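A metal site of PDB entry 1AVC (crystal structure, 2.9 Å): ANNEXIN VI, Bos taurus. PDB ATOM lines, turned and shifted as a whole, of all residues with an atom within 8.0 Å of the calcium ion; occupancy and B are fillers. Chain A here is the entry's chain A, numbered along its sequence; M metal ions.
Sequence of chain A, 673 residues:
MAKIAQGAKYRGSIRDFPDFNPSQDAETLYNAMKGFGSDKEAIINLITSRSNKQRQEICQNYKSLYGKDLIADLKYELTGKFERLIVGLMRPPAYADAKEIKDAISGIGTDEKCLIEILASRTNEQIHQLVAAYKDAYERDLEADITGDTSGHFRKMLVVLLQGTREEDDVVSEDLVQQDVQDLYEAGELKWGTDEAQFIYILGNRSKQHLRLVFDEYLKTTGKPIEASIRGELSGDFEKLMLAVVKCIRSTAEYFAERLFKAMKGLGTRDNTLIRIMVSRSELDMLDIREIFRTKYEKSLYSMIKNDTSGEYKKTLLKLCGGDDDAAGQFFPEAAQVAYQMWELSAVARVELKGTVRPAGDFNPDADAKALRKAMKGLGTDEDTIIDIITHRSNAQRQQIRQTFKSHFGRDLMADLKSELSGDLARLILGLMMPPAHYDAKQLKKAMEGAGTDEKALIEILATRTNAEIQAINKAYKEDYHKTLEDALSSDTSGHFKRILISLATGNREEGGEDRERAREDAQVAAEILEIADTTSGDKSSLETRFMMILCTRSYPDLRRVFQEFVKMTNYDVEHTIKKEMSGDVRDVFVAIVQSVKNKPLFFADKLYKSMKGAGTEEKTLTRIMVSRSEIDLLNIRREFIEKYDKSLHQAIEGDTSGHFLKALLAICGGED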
ATOM      1  N   ARG A 373     -14.721 -14.670   6.615  1.00  0.00           N
ATOM      2  CA  ARG A 373     -15.493 -13.885   5.655  1.00  0.00           C
ATOM      3  C   ARG A 373     -14.645 -13.542   4.432  1.00  0.00           C
ATOM      4  O   ARG A 373     -15.127 -13.595   3.294  1.00  0.00           O
ATOM      5  CB  ARG A 373     -15.984 -12.592   6.314  1.00  0.00           C
ATOM      6  CG  ARG A 373     -16.500 -11.550   5.341  1.00  0.00           C
ATOM      7  CD  ARG A 373     -18.018 -11.621   5.209  1.00  0.00           C
ATOM      8  NE  ARG A 373     -18.515 -10.734   4.167  1.00  0.00           N
ATOM      9  CZ  ARG A 373     -19.667 -10.906   3.526  1.00  0.00           C
ATOM     10  NH1 ARG A 373     -20.441 -11.952   3.818  1.00  0.00           N
ATOM     11  NH2 ARG A 373     -20.051 -10.047   2.590  1.00  0.00           N
ATOM     12  N   LYS A 374     -13.378 -13.212   4.669  1.00  0.00           N
ATOM     13  CA  LYS A 374     -12.459 -12.866   3.605  1.00  0.00           C
ATOM     14  C   LYS A 374     -12.168 -14.058   2.693  1.00  0.00           C
ATOM     15  O   LYS A 374     -12.142 -13.923   1.466  1.00  0.00           O
ATOM     16  CB  LYS A 374     -11.143 -12.347   4.193  1.00  0.00           C
ATOM     17  CG  LYS A 374     -10.044 -12.066   3.172  1.00  0.00           C
ATOM     18  CD  LYS A 374      -9.164 -13.298   2.940  1.00  0.00           C
ATOM     19  CE  LYS A 374      -8.458 -13.735   4.214  1.00  0.00           C
ATOM     20  NZ  LYS A 374      -7.714 -15.002   4.019  1.00  0.00           N
ATOM     21  N   ALA A 375     -11.949 -15.223   3.294  1.00  0.00           N
ATOM     22  CA  ALA A 375     -11.635 -16.436   2.551  1.00  0.00           C
ATOM     23  C   ALA A 375     -12.828 -17.039   1.812  1.00  0.00           C
ATOM     24  O   ALA A 375     -12.706 -18.099   1.198  1.00  0.00           O
ATOM     25  CB  ALA A 375     -11.038 -17.473   3.490  1.00  0.00           C
ATOM     26  N   MET A 376     -13.977 -16.372   1.855  1.00  0.00           N
ATOM     27  CA  MET A 376     -15.163 -16.871   1.184  1.00  0.00           C
ATOM     28  C   MET A 376     -15.647 -15.920   0.093  1.00  0.00           C
ATOM     29  O   MET A 376     -16.446 -16.294  -0.766  1.00  0.00           O
ATOM     30  CB  MET A 376     -16.285 -17.107   2.198  1.00  0.00           C
ATOM     31  CG  MET A 376     -16.040 -18.282   3.129  1.00  0.00           C
ATOM     32  SD  MET A 376     -17.486 -18.698   4.115  1.00  0.00           S
ATOM     33  CE  MET A 376     -17.109 -17.875   5.650  1.00  0.00           C
ATOM     34  N   LYS A 377     -15.154 -14.681   0.133  1.00  0.00           N
ATOM     35  CA  LYS A 377     -15.540 -13.674  -0.847  1.00  0.00           C
ATOM     36  C   LYS A 377     -14.900 -13.968  -2.197  1.00  0.00           C
ATOM     37  O   LYS A 377     -13.798 -14.530  -2.267  1.00  0.00           O
ATOM     38  CB  LYS A 377     -15.123 -12.288  -0.368  1.00  0.00           C
ATOM     39  CG  LYS A 377     -16.277 -11.421   0.104  1.00  0.00           C
ATOM     40  CD  LYS A 377     -16.078 -10.969   1.549  1.00  0.00           C
ATOM     41  CE  LYS A 377     -16.283  -9.467   1.689  1.00  0.00           C
ATOM     42  NZ  LYS A 377     -15.269  -8.851   2.597  1.00  0.00           N
ATOM     43  N   GLY A 378     -15.581 -13.581  -3.275  1.00  0.00           N
ATOM     44  CA  GLY A 378     -15.069 -13.811  -4.615  1.00  0.00           C
ATOM     45  C   GLY A 378     -15.720 -15.036  -5.219  1.00  0.00           C
ATOM     46  O   GLY A 378     -16.672 -15.575  -4.663  1.00  0.00           O
ATOM     47  N   LEU A 379     -15.215 -15.488  -6.370  1.00  0.00           N
ATOM     48  CA  LEU A 379     -15.775 -16.677  -7.004  1.00  0.00           C
ATOM     49  C   LEU A 379     -15.290 -17.913  -6.256  1.00  0.00           C
ATOM     50  O   LEU A 379     -16.102 -18.682  -5.730  1.00  0.00           O
ATOM     51  CB  LEU A 379     -15.341 -16.764  -8.476  1.00  0.00           C
ATOM     52  CG  LEU A 379     -16.118 -17.798  -9.304  1.00  0.00           C
ATOM     53  CD1 LEU A 379     -17.590 -17.421  -9.335  1.00  0.00           C
ATOM     54  CD2 LEU A 379     -15.553 -17.877 -10.706  1.00  0.00           C
ATOM     55  N   GLY A 380     -13.975 -18.087  -6.222  1.00  0.00           N
ATOM     56  CA  GLY A 380     -13.382 -19.214  -5.531  1.00  0.00           C
ATOM     57  C   GLY A 380     -13.417 -19.020  -4.031  1.00  0.00           C
ATOM     58  O   GLY A 380     -13.614 -17.905  -3.542  1.00  0.00           O
ATOM     59  N   THR A 381     -13.213 -20.098  -3.287  1.00  0.00           N
ATOM     60  CA  THR A 381     -13.230 -20.038  -1.832  1.00  0.00           C
ATOM     61  C   THR A 381     -11.898 -20.469  -1.232  1.00  0.00           C
ATOM     62  O   THR A 381     -11.462 -21.602  -1.424  1.00  0.00           O
ATOM     63  CB  THR A 381     -14.352 -20.941  -1.268  1.00  0.00           C
ATOM     64  OG1 THR A 381     -13.914 -21.548  -0.047  1.00  0.00           O
ATOM     65  CG2 THR A 381     -14.703 -22.024  -2.272  1.00  0.00           C
ATOM     66  N   ASP A 382     -11.251 -19.567  -0.506  1.00  0.00           N
ATOM     67  CA  ASP A 382      -9.966 -19.865   0.126  1.00  0.00           C
ATOM     68  C   ASP A 382     -10.221 -20.889   1.235  1.00  0.00           C
ATOM     69  O   ASP A 382     -10.552 -20.537   2.360  1.00  0.00           O
ATOM     70  CB  ASP A 382      -9.369 -18.598   0.724  1.00  0.00           C
ATOM     71  CG  ASP A 382      -8.070 -18.851   1.478  1.00  0.00           C
ATOM     72  OD1 ASP A 382      -7.622 -20.017   1.516  1.00  0.00           O
ATOM     73  OD2 ASP A 382      -7.512 -17.883   2.034  1.00  0.00           O
ATOM     74  N   SER A 419     -22.592 -23.202   1.608  1.00  0.00           N
ATOM     75  CA  SER A 419     -22.644 -22.789   0.204  1.00  0.00           C
ATOM     76  C   SER A 419     -21.279 -22.652  -0.468  1.00  0.00           C
ATOM     77  O   SER A 419     -21.131 -22.999  -1.642  1.00  0.00           O
ATOM     78  CB  SER A 419     -23.407 -21.473   0.083  1.00  0.00           C
ATOM     79  OG  SER A 419     -22.739 -20.560  -0.762  1.00  0.00           O
ATOM     80  N   GLU A 420     -20.288 -22.148   0.259  1.00  0.00           N
ATOM     81  CA  GLU A 420     -18.961 -21.959  -0.308  1.00  0.00           C
ATOM     82  C   GLU A 420     -18.103 -23.228  -0.294  1.00  0.00           C
ATOM     83  O   GLU A 420     -17.106 -23.320  -1.014  1.00  0.00           O
ATOM     84  CB  GLU A 420     -18.255 -20.825   0.414  1.00  0.00           C
ATOM     85  CG  GLU A 420     -18.693 -19.471  -0.075  1.00  0.00           C
ATOM     86  CD  GLU A 420     -17.948 -19.084  -1.328  1.00  0.00           C
ATOM     87  OE1 GLU A 420     -16.709 -19.148  -1.299  1.00  0.00           O
ATOM     88  OE2 GLU A 420     -18.592 -18.733  -2.331  1.00  0.00           O
ATOM     89  N   LEU A 421     -18.492 -24.202   0.527  1.00  0.00           N
ATOM     90  CA  LEU A 421     -17.746 -25.462   0.607  1.00  0.00           C
ATOM     91  C   LEU A 421     -18.547 -26.600  -0.019  1.00  0.00           C
ATOM     92  O   LEU A 421     -19.771 -26.505  -0.165  1.00  0.00           O
ATOM     93  CB  LEU A 421     -17.441 -25.799   2.066  1.00  0.00           C
ATOM     94  CG  LEU A 421     -16.385 -24.942   2.787  1.00  0.00           C
ATOM     95  CD1 LEU A 421     -16.020 -25.597   4.113  1.00  0.00           C
ATOM     96  CD2 LEU A 421     -15.147 -24.800   1.910  1.00  0.00           C
HETATM   97 CA    CA M   1     -16.055 -17.884  -3.336  1.00  0.00          CA
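O of Gly 380 binds the calcium ion. OE1 of Glu 420 is bound to the calcium ion, 2.5 Å away. The calcium ion is bound by O of Leu 379 (2.5 Å). O of Gly 378 binds the calcium ion, 2.7 Å away. The side-chain carboxylate (OE2) of Glu 420 binds the calcium ion. Slightly farther from the calcium ion lies the backbone carbonyl oxygen (O) of Met 376 (3.0 Å).
Residues that only touch the calcium ion: Thr 381. The nearest printed residue that does not touch the calcium ion is Lys 377 (4.2 Å).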
